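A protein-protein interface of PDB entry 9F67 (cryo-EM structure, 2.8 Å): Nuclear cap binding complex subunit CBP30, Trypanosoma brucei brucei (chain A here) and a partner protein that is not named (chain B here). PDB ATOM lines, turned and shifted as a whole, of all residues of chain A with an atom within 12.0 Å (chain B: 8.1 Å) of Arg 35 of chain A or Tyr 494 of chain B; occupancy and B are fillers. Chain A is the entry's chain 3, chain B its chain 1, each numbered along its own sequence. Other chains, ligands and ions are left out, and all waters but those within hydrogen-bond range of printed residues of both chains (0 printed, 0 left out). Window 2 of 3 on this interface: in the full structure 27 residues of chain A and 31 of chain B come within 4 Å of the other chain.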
ATOM      1  N   GLN A  31      20.963  42.798  20.001  1.00  0.00           N
ATOM      2  CA  GLN A  31      22.207  42.058  20.174  1.00  0.00           C
ATOM      3  C   GLN A  31      21.887  40.576  20.017  1.00  0.00           C
ATOM      4  O   GLN A  31      20.796  40.193  19.580  1.00  0.00           O
ATOM      5  CB  GLN A  31      22.867  42.374  21.528  1.00  0.00           C
ATOM      6  CG  GLN A  31      22.953  43.854  21.889  1.00  0.00           C
ATOM      7  CD  GLN A  31      21.672  44.385  22.503  1.00  0.00           C
ATOM      8  OE1 GLN A  31      20.669  43.677  22.587  1.00  0.00           O
ATOM      9  NE2 GLN A  31      21.701  45.640  22.937  1.00  0.00           N
ATOM     10  N   LYS A  32      22.847  39.723  20.367  1.00  0.00           N
ATOM     11  CA  LYS A  32      22.618  38.286  20.342  1.00  0.00           C
ATOM     12  C   LYS A  32      21.614  37.892  21.417  1.00  0.00           C
ATOM     13  O   LYS A  32      21.637  38.418  22.533  1.00  0.00           O
ATOM     14  CB  LYS A  32      23.932  37.533  20.544  1.00  0.00           C
ATOM     15  CG  LYS A  32      24.990  37.843  19.497  1.00  0.00           C
ATOM     16  CD  LYS A  32      24.447  37.657  18.089  1.00  0.00           C
ATOM     17  CE  LYS A  32      24.574  38.935  17.277  1.00  0.00           C
ATOM     18  NZ  LYS A  32      24.011  38.779  15.907  1.00  0.00           N
ATOM     19  N   ARG A  33      20.729  36.954  21.078  1.00  0.00           N
ATOM     20  CA  ARG A  33      19.647  36.549  21.967  1.00  0.00           C
ATOM     21  C   ARG A  33      19.771  35.097  22.410  1.00  0.00           C
ATOM     22  O   ARG A  33      18.808  34.536  22.942  1.00  0.00           O
ATOM     23  CB  ARG A  33      18.291  36.779  21.298  1.00  0.00           C
ATOM     24  CG  ARG A  33      18.064  38.201  20.828  1.00  0.00           C
ATOM     25  CD  ARG A  33      16.585  38.498  20.684  1.00  0.00           C
ATOM     26  NE  ARG A  33      15.859  38.250  21.923  1.00  0.00           N
ATOM     27  CZ  ARG A  33      14.550  38.404  22.067  1.00  0.00           C
ATOM     28  NH1 ARG A  33      13.787  38.804  21.062  1.00  0.00           N
ATOM     29  NH2 ARG A  33      13.993  38.153  23.248  1.00  0.00           N
ATOM     30  N   ARG A  34      20.936  34.482  22.212  1.00  0.00           N
ATOM     31  CA  ARG A  34      21.185  33.080  22.571  1.00  0.00           C
ATOM     32  C   ARG A  34      20.126  32.228  21.873  1.00  0.00           C
ATOM     33  O   ARG A  34      19.776  32.520  20.721  1.00  0.00           O
ATOM     34  CB  ARG A  34      21.238  32.946  24.086  1.00  0.00           C
ATOM     35  CG  ARG A  34      22.346  32.043  24.590  1.00  0.00           C
ATOM     36  CD  ARG A  34      22.645  32.303  26.059  1.00  0.00           C
ATOM     37  NE  ARG A  34      21.427  32.418  26.851  1.00  0.00           N
ATOM     38  CZ  ARG A  34      21.402  32.672  28.153  1.00  0.00           C
ATOM     39  NH1 ARG A  34      22.516  32.845  28.846  1.00  0.00           N
ATOM     40  NH2 ARG A  34      20.229  32.755  28.776  1.00  0.00           N
ATOM     41  N   ARG A  35      19.584  31.226  22.573  1.00  0.00           N
ATOM     42  CA  ARG A  35      18.498  30.394  21.988  1.00  0.00           C
ATOM     43  C   ARG A  35      17.342  30.267  22.996  1.00  0.00           C
ATOM     44  O   ARG A  35      16.173  30.221  22.553  1.00  0.00           O
ATOM     45  CB  ARG A  35      19.017  29.008  21.586  1.00  0.00           C
ATOM     46  CG  ARG A  35      17.986  28.174  20.839  1.00  0.00           C
ATOM     47  CD  ARG A  35      18.468  26.767  20.521  1.00  0.00           C
ATOM     48  NE  ARG A  35      17.422  25.973  19.867  1.00  0.00           N
ATOM     49  CZ  ARG A  35      17.555  24.708  19.491  1.00  0.00           C
ATOM     50  NH1 ARG A  35      18.682  24.062  19.729  1.00  0.00           N
ATOM     51  NH2 ARG A  35      16.558  24.091  18.881  1.00  0.00           N
ATOM     52  N   GLU A  36      17.655  30.228  24.294  1.00  0.00           N
ATOM     53  CA  GLU A  36      16.606  30.041  25.333  1.00  0.00           C
ATOM     54  C   GLU A  36      15.971  31.394  25.697  1.00  0.00           C
ATOM     55  O   GLU A  36      15.089  31.411  26.583  1.00  0.00           O
ATOM     56  CB  GLU A  36      17.211  29.365  26.564  1.00  0.00           C
ATOM     57  CG  GLU A  36      18.584  29.917  26.935  1.00  0.00           C
ATOM     58  CD  GLU A  36      19.124  29.384  28.249  1.00  0.00           C
ATOM     59  OE1 GLU A  36      18.398  28.615  28.914  1.00  0.00           O
ATOM     60  OE2 GLU A  36      20.269  29.730  28.605  1.00  0.00           O
ATOM     61  N   GLU A  37      16.401  32.476  25.043  1.00  0.00           N
ATOM     62  CA  GLU A  37      15.847  33.827  25.326  1.00  0.00           C
ATOM     63  C   GLU A  37      15.002  34.278  24.124  1.00  0.00           C
ATOM     64  O   GLU A  37      14.426  35.386  24.180  1.00  0.00           O
ATOM     65  CB  GLU A  37      17.004  34.776  25.641  1.00  0.00           C
ATOM     66  CG  GLU A  37      16.575  36.070  26.326  1.00  0.00           C
ATOM     67  CD  GLU A  37      16.560  37.284  25.416  1.00  0.00           C
ATOM     68  OE1 GLU A  37      16.917  37.136  24.229  1.00  0.00           O
ATOM     69  OE2 GLU A  37      16.186  38.377  25.891  1.00  0.00           O
ATOM     70  N   CYS A  38      14.911  33.440  23.087  1.00  0.00           N
ATOM     71  CA  CYS A  38      14.168  33.801  21.887  1.00  0.00           C
ATOM     72  C   CYS A  38      12.932  32.931  21.690  1.00  0.00           C
ATOM     73  O   CYS A  38      12.378  32.905  20.585  1.00  0.00           O
ATOM     74  CB  CYS A  38      15.063  33.703  20.652  1.00  0.00           C
ATOM     75  SG  CYS A  38      15.474  32.018  20.172  1.00  0.00           S
ATOM     76  N   VAL A  39      12.448  32.334  22.793  1.00  0.00           N
ATOM     77  CA  VAL A  39      11.291  31.400  22.840  1.00  0.00           C
ATOM     78  C   VAL A  39      10.076  32.131  23.360  1.00  0.00           C
ATOM     79  O   VAL A  39      10.029  32.404  24.540  1.00  0.00           O
ATOM     80  CB  VAL A  39      11.488  30.164  23.722  1.00  0.00           C
ATOM     81  CG1 VAL A  39      12.295  29.099  23.003  1.00  0.00           C
ATOM     82  CG2 VAL A  39      12.153  30.491  25.040  1.00  0.00           C
ATOM     83  N   VAL A  40       9.089  32.347  22.510  1.00  0.00           N
ATOM     84  CA  VAL A  40       7.885  32.966  23.044  1.00  0.00           C
ATOM     85  C   VAL A  40       6.736  31.977  22.919  1.00  0.00           C
ATOM     86  O   VAL A  40       6.456  31.465  21.829  1.00  0.00           O
ATOM     87  CB  VAL A  40       7.584  34.281  22.316  1.00  0.00           C
ATOM     88  CG1 VAL A  40       6.577  35.081  23.087  1.00  0.00           C
ATOM     89  CG2 VAL A  40       8.854  35.077  22.141  1.00  0.00           C
ATOM     90  N   LEU A  41       6.074  31.713  24.020  1.00  0.00           N
ATOM     91  CA  LEU A  41       5.130  30.624  24.178  1.00  0.00           C
ATOM     92  C   LEU A  41       3.741  31.019  23.696  1.00  0.00           C
ATOM     93  O   LEU A  41       3.421  32.206  23.591  1.00  0.00           O
ATOM     94  CB  LEU A  41       5.083  30.200  25.647  1.00  0.00           C
ATOM     95  CG  LEU A  41       6.227  29.276  26.051  1.00  0.00           C
ATOM     96  CD1 LEU A  41       6.037  28.783  27.465  1.00  0.00           C
ATOM     97  CD2 LEU A  41       6.325  28.110  25.097  1.00  0.00           C
ATOM     98  N   PRO A  77      13.749  30.915  35.050  1.00  0.00           N
ATOM     99  CA  PRO A  77      13.348  32.032  34.222  1.00  0.00           C
ATOM    100  C   PRO A  77      12.440  31.414  33.181  1.00  0.00           C
ATOM    101  O   PRO A  77      12.917  30.676  32.385  1.00  0.00           O
ATOM    102  CB  PRO A  77      14.595  32.523  33.522  1.00  0.00           C
ATOM    103  CG  PRO A  77      15.716  31.768  34.191  1.00  0.00           C
ATOM    104  CD  PRO A  77      15.080  30.474  34.652  1.00  0.00           C
ATOM    105  N   ILE A  78      11.176  31.785  33.182  1.00  0.00           N
ATOM    106  CA  ILE A  78      10.203  31.056  32.347  1.00  0.00           C
ATOM    107  C   ILE A  78       9.826  31.955  31.209  1.00  0.00           C
ATOM    108  O   ILE A  78       9.529  33.103  31.456  1.00  0.00           O
ATOM    109  CB  ILE A  78       9.046  30.428  33.154  1.00  0.00           C
ATOM    110  CG1 ILE A  78       8.290  31.469  33.977  1.00  0.00           C
ATOM    111  CG2 ILE A  78       9.527  29.293  34.036  1.00  0.00           C
ATOM    112  CD1 ILE A  78       7.173  30.883  34.804  1.00  0.00           C
ATOM    113  N   LEU A  79       9.726  31.326  30.038  1.00  0.00           N
ATOM    114  CA  LEU A  79       9.517  32.009  28.745  1.00  0.00           C
ATOM    115  C   LEU A  79       8.266  32.869  28.704  1.00  0.00           C
ATOM    116  O   LEU A  79       7.250  32.489  29.314  1.00  0.00           O
ATOM    117  CB  LEU A  79       9.280  30.872  27.750  1.00  0.00           C
ATOM    118  CG  LEU A  79      10.091  29.591  27.949  1.00  0.00           C
ATOM    119  CD1 LEU A  79       9.902  28.674  26.757  1.00  0.00           C
ATOM    120  CD2 LEU A  79      11.572  29.849  28.204  1.00  0.00           C
ATOM    121  N   PRO A  80       8.218  33.975  27.905  1.00  0.00           N
ATOM    122  CA  PRO A  80       7.005  34.805  27.790  1.00  0.00           C
ATOM    123  C   PRO A  80       5.874  34.257  26.905  1.00  0.00           C
ATOM    124  O   PRO A  80       6.159  33.617  25.913  1.00  0.00           O
ATOM    125  CB  PRO A  80       7.511  36.113  27.160  1.00  0.00           C
ATOM    126  CG  PRO A  80       8.646  35.671  26.280  1.00  0.00           C
ATOM    127  CD  PRO A  80       9.295  34.551  27.063  1.00  0.00           C
ATOM    128  N   PHE B 446       7.445  21.994  28.551  1.00  0.00           N
ATOM    129  CA  PHE B 446       8.329  21.274  29.506  1.00  0.00           C
ATOM    130  C   PHE B 446       8.176  21.935  30.874  1.00  0.00           C
ATOM    131  O   PHE B 446       8.995  21.667  31.772  1.00  0.00           O
ATOM    132  CB  PHE B 446       9.773  21.245  28.996  1.00  0.00           C
ATOM    133  CG  PHE B 446       9.944  20.553  27.667  1.00  0.00           C
ATOM    134  CD1 PHE B 446       9.602  19.220  27.515  1.00  0.00           C
ATOM    135  CD2 PHE B 446      10.421  21.241  26.564  1.00  0.00           C
ATOM    136  CE1 PHE B 446       9.763  18.580  26.296  1.00  0.00           C
ATOM    137  CE2 PHE B 446      10.568  20.603  25.342  1.00  0.00           C
ATOM    138  CZ  PHE B 446      10.244  19.273  25.211  1.00  0.00           C
ATOM    139  N   VAL B 489      12.596  13.623  27.956  1.00  0.00           N
ATOM    140  CA  VAL B 489      12.310  15.009  27.608  1.00  0.00           C
ATOM    141  C   VAL B 489      13.502  15.643  26.900  1.00  0.00           C
ATOM    142  O   VAL B 489      13.338  16.402  25.939  1.00  0.00           O
ATOM    143  CB  VAL B 489      11.907  15.795  28.869  1.00  0.00           C
ATOM    144  CG1 VAL B 489      12.158  17.274  28.685  1.00  0.00           C
ATOM    145  CG2 VAL B 489      10.454  15.543  29.204  1.00  0.00           C
ATOM    146  N   ALA B 490      14.719  15.331  27.352  1.00  0.00           N
ATOM    147  CA  ALA B 490      15.914  15.966  26.808  1.00  0.00           C
ATOM    148  C   ALA B 490      16.140  15.647  25.337  1.00  0.00           C
ATOM    149  O   ALA B 490      16.864  16.387  24.664  1.00  0.00           O
ATOM    150  CB  ALA B 490      17.145  15.556  27.613  1.00  0.00           C
ATOM    151  N   ARG B 491      15.559  14.564  24.823  1.00  0.00           N
ATOM    152  CA  ARG B 491      15.680  14.281  23.399  1.00  0.00           C
ATOM    153  C   ARG B 491      14.904  15.283  22.559  1.00  0.00           C
ATOM    154  O   ARG B 491      15.291  15.569  21.422  1.00  0.00           O
ATOM    155  CB  ARG B 491      15.193  12.871  23.092  1.00  0.00           C
ATOM    156  CG  ARG B 491      16.107  11.777  23.566  1.00  0.00           C
ATOM    157  CD  ARG B 491      15.337  10.493  23.743  1.00  0.00           C
ATOM    158  NE  ARG B 491      15.963   9.622  24.726  1.00  0.00           N
ATOM    159  CZ  ARG B 491      15.378   8.559  25.259  1.00  0.00           C
ATOM    160  NH1 ARG B 491      14.147   8.211  24.927  1.00  0.00           N
ATOM    161  NH2 ARG B 491      16.045   7.830  26.149  1.00  0.00           N
ATOM    162  N   ARG B 492      13.907  15.915  23.099  1.00  0.00           N
ATOM    163  CA  ARG B 492      13.043  16.757  22.281  1.00  0.00           C
ATOM    164  C   ARG B 492      13.347  18.196  22.553  1.00  0.00           C
ATOM    165  O   ARG B 492      12.614  19.040  22.066  1.00  0.00           O
ATOM    166  CB  ARG B 492      11.662  16.486  22.839  1.00  0.00           C
ATOM    167  CG  ARG B 492      11.135  15.065  22.820  1.00  0.00           C
ATOM    168  CD  ARG B 492       9.743  15.011  23.360  1.00  0.00           C
ATOM    169  NE  ARG B 492       9.298  13.625  23.254  1.00  0.00           N
ATOM    170  CZ  ARG B 492       8.264  13.229  22.546  1.00  0.00           C
ATOM    171  NH1 ARG B 492       7.687  14.051  21.698  1.00  0.00           N
ATOM    172  NH2 ARG B 492       7.809  12.003  22.686  1.00  0.00           N
ATOM    173  N   THR B 493      14.381  18.467  23.357  1.00  0.00           N
ATOM    174  CA  THR B 493      14.716  19.859  23.733  1.00  0.00           C
ATOM    175  C   THR B 493      16.217  19.990  23.871  1.00  0.00           C
ATOM    176  O   THR B 493      16.931  19.043  23.478  1.00  0.00           O
ATOM    177  CB  THR B 493      13.992  20.230  25.027  1.00  0.00           C
ATOM    178  OG1 THR B 493      14.243  21.619  25.215  1.00  0.00           O
ATOM    179  CG2 THR B 493      14.494  19.444  26.225  1.00  0.00           C
ATOM    180  N   TYR B 494      16.689  21.130  24.386  1.00  0.00           N
ATOM    181  CA  TYR B 494      18.149  21.335  24.600  1.00  0.00           C
ATOM    182  C   TYR B 494      18.408  21.481  26.102  1.00  0.00           C
ATOM    183  O   TYR B 494      17.469  21.837  26.849  1.00  0.00           O
ATOM    184  CB  TYR B 494      18.657  22.507  23.751  1.00  0.00           C
ATOM    185  CG  TYR B 494      17.829  23.785  23.791  1.00  0.00           C
ATOM    186  CD1 TYR B 494      16.723  23.948  22.966  1.00  0.00           C
ATOM    187  CD2 TYR B 494      18.180  24.845  24.618  1.00  0.00           C
ATOM    188  CE1 TYR B 494      15.971  25.111  22.987  1.00  0.00           C
ATOM    189  CE2 TYR B 494      17.439  26.016  24.644  1.00  0.00           C
ATOM    190  CZ  TYR B 494      16.332  26.148  23.828  1.00  0.00           C
ATOM    191  OH  TYR B 494      15.593  27.296  23.846  1.00  0.00           O
ATOM    192  N   GLY B 495      19.635  21.178  26.537  1.00  0.00           N
ATOM    193  CA  GLY B 495      19.970  21.247  27.973  1.00  0.00           C
ATOM    194  C   GLY B 495      19.587  22.589  28.563  1.00  0.00           C
ATOM    195  O   GLY B 495      18.954  22.598  29.636  1.00  0.00           O
ATOM    196  N   LEU B 496      19.938  23.684  27.881  1.00  0.00           N
ATOM    197  CA  LEU B 496      19.659  25.042  28.413  1.00  0.00           C
ATOM    198  C   LEU B 496      18.157  25.182  28.698  1.00  0.00           C
ATOM    199  O   LEU B 496      17.809  25.658  29.797  1.00  0.00           O
ATOM    200  CB  LEU B 496      20.131  26.089  27.405  1.00  0.00           C
ATOM    201  CG  LEU B 496      21.629  26.093  27.093  1.00  0.00           C
ATOM    202  CD1 LEU B 496      21.950  27.164  26.066  1.00  0.00           C
ATOM    203  CD2 LEU B 496      22.434  26.312  28.363  1.00  0.00           C
ATOM    204  N   ARG B 497      17.310  24.770  27.752  1.00  0.00           N
ATOM    205  CA  ARG B 497      15.841  24.914  27.918  1.00  0.00           C
ATOM    206  C   ARG B 497      15.400  24.176  29.191  1.00  0.00           C
ATOM    207  O   ARG B 497      14.718  24.798  30.037  1.00  0.00           O
ATOM    208  CB  ARG B 497      15.144  24.347  26.677  1.00  0.00           C
ATOM    209  CG  ARG B 497      13.629  24.474  26.644  1.00  0.00           C
ATOM    210  CD  ARG B 497      13.166  25.917  26.748  1.00  0.00           C
ATOM    211  NE  ARG B 497      11.754  26.058  26.376  1.00  0.00           N
ATOM    212  CZ  ARG B 497      10.738  25.451  26.977  1.00  0.00           C
ATOM    213  NH1 ARG B 497       9.558  25.406  26.385  1.00  0.00           N
ATOM    214  NH2 ARG B 497      10.898  24.892  28.163  1.00  0.00           N
ATOM    215  N   LEU B 498      15.798  22.907  29.324  1.00  0.00           N
ATOM    216  CA  LEU B 498      15.412  22.109  30.516  1.00  0.00           C
ATOM    217  C   LEU B 498      15.982  22.780  31.773  1.00  0.00           C
ATOM    218  O   LEU B 498      15.202  23.014  32.717  1.00  0.00           O
ATOM    219  CB  LEU B 498      15.917  20.674  30.375  1.00  0.00           C
ATOM    220  CG  LEU B 498      14.856  19.627  30.026  1.00  0.00           C
ATOM    221  CD1 LEU B 498      15.428  18.224  30.119  1.00  0.00           C
ATOM    222  CD2 LEU B 498      13.650  19.781  30.938  1.00  0.00           C
ATOM    223  N   ARG B 499      17.277  23.108  31.766  1.00  0.00           N
ATOM    224  CA  ARG B 499      17.927  23.701  32.965  1.00  0.00           C
ATOM    225  C   ARG B 499      17.242  25.031  33.324  1.00  0.00           C
ATOM    226  O   ARG B 499      17.115  25.321  34.532  1.00  0.00           O
ATOM    227  CB  ARG B 499      19.429  23.874  32.714  1.00  0.00           C
ATOM    228  CG  ARG B 499      20.171  22.544  32.673  1.00  0.00           C
ATOM    229  CD  ARG B 499      21.628  22.704  32.268  1.00  0.00           C
ATOM    230  NE  ARG B 499      22.410  21.473  32.437  1.00  0.00           N
ATOM    231  CZ  ARG B 499      22.662  20.876  33.597  1.00  0.00           C
ATOM    232  NH1 ARG B 499      22.411  21.498  34.735  1.00  0.00           N
ATOM    233  NH2 ARG B 499      23.183  19.662  33.615  1.00  0.00           N
ATOM    234  N   ALA B 500      16.825  25.804  32.317  1.00  0.00           N
ATOM    235  CA  ALA B 500      16.168  27.106  32.575  1.00  0.00           C
ATOM    236  C   ALA B 500      14.892  26.882  33.390  1.00  0.00           C
ATOM    237  O   ALA B 500      14.704  27.563  34.420  1.00  0.00           O
ATOM    238  CB  ALA B 500      15.871  27.808  31.268  1.00  0.00           C
ATOM    239  N   ILE B 501      14.047  25.948  32.945  1.00  0.00           N
ATOM    240  CA  ILE B 501      12.762  25.672  33.658  1.00  0.00           C
ATOM    241  C   ILE B 501      13.065  24.902  34.956  1.00  0.00           C
ATOM    242  O   ILE B 501      12.521  25.293  36.013  1.00  0.00           O
ATOM    243  CB  ILE B 501      11.778  24.908  32.750  1.00  0.00           C
ATOM    244  CG1 ILE B 501      10.985  25.856  31.846  1.00  0.00           C
ATOM    245  CG2 ILE B 501      10.845  24.026  33.578  1.00  0.00           C
ATOM    246  CD1 ILE B 501      11.825  26.635  30.850  1.00  0.00           C
ATOM    247  N   PHE B 514      23.014  15.386  31.796  1.00  0.00           N
ATOM    248  CA  PHE B 514      23.611  16.301  30.833  1.00  0.00           C
ATOM    249  C   PHE B 514      25.125  16.369  30.999  1.00  0.00           C
ATOM    250  O   PHE B 514      25.664  16.033  32.053  1.00  0.00           O
ATOM    251  CB  PHE B 514      23.005  17.697  30.976  1.00  0.00           C
ATOM    252  CG  PHE B 514      21.611  17.805  30.445  1.00  0.00           C
ATOM    253  CD1 PHE B 514      21.314  17.399  29.155  1.00  0.00           C
ATOM    254  CD2 PHE B 514      20.595  18.315  31.232  1.00  0.00           C
ATOM    255  CE1 PHE B 514      20.028  17.498  28.661  1.00  0.00           C
ATOM    256  CE2 PHE B 514      19.307  18.418  30.745  1.00  0.00           C
ATOM    257  CZ  PHE B 514      19.023  18.010  29.457  1.00  0.00           C
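Among the printed residues, merely in contact across the chains: Pro 77 of chain A with Ala 500 of chain B (2.9 Å), Leu 79 of chain A with Arg 497 of chain B (3.2 Å), Glu 36 of chain A with Tyr 494 of chain B (3.3 Å), Glu 36 of chain A with Ala 500 of chain B (3.5 Å) and Val 39 of chain A with Tyr 494 of chain B (3.9 Å).
The backbone carbonyl oxygen (O) of Arg 35 of chain A lies within hydrogen-bond range of the side-chain hydroxyl (OH) of Tyr 494 of chain B, 3.3 Å away.
The backbone carbonyl oxygen of Leu 496 of chain B sits close to the side-chain carboxylate of Glu 36 of chain A (3.1 Å).
Of the 15 printed residues of chain B, 4 touch a printed residue of chain A.
Hydrophobic or aromatic side chains of chain A within 4 Å of the printed part of chain B: Val 39, Pro 77 and Leu 79.
Among the printed residues, no Asp or Glu carboxylate lies within 4 Å of a Lys or Arg side-chain nitrogen of the other chain.
Of chain B, only Tyr 494 comes within 4 Å of Arg 35 of chain A.
Of the printed residues of chain B, Glu 36 of chain A touches Tyr 494, Leu 496 and Ala 500.
Printed residues of chain B within 4 Å of Val 39 of chain A: Tyr 494.
Leu 41 of chain A touches none of the printed residues of chain B.
Of the printed residues of chain B, Pro 77 of chain A touches Ala 500 (2.9 Å).
Ile 78 of chain A touches none of the printed residues of chain B.
Of the printed residues of chain B, Leu 79 of chain A touches Arg 497.
No residue of chain A comes within 4 Å of Ala 490 of chain B.
Tyr 494 of chain B touches just these residues of chain A: Arg 35 (3.3 Å), Glu 36 (3.3 Å) and Val 39 (3.9 Å).
Leu 496 of chain B touches just one residue of chain A: Glu 36.
Of the printed residues of chain A, Arg 497 of chain B touches Leu 79.
No residue of chain A comes within 4 Å of Leu 498 of chain B.
Of the printed residues of chain A, Ala 500 of chain B touches Glu 36 (3.5 Å) and Pro 77 (2.9 Å).
The nearest printed residue of chain B that does not touch Val 39 of chain A is Arg 497 of chain B (4.6 Å).
The guanidinium group (NH2) of Arg 34 of chain A lies within salt-bridge range of the side-chain carboxylate (OE2) of Glu 36 of chain A, 3.0 Å away.
The backbone carbonyl oxygen of Arg 35 of chain A is in hydrogen-bond range of the side-chain sulfur of Cys 38 of chain A.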
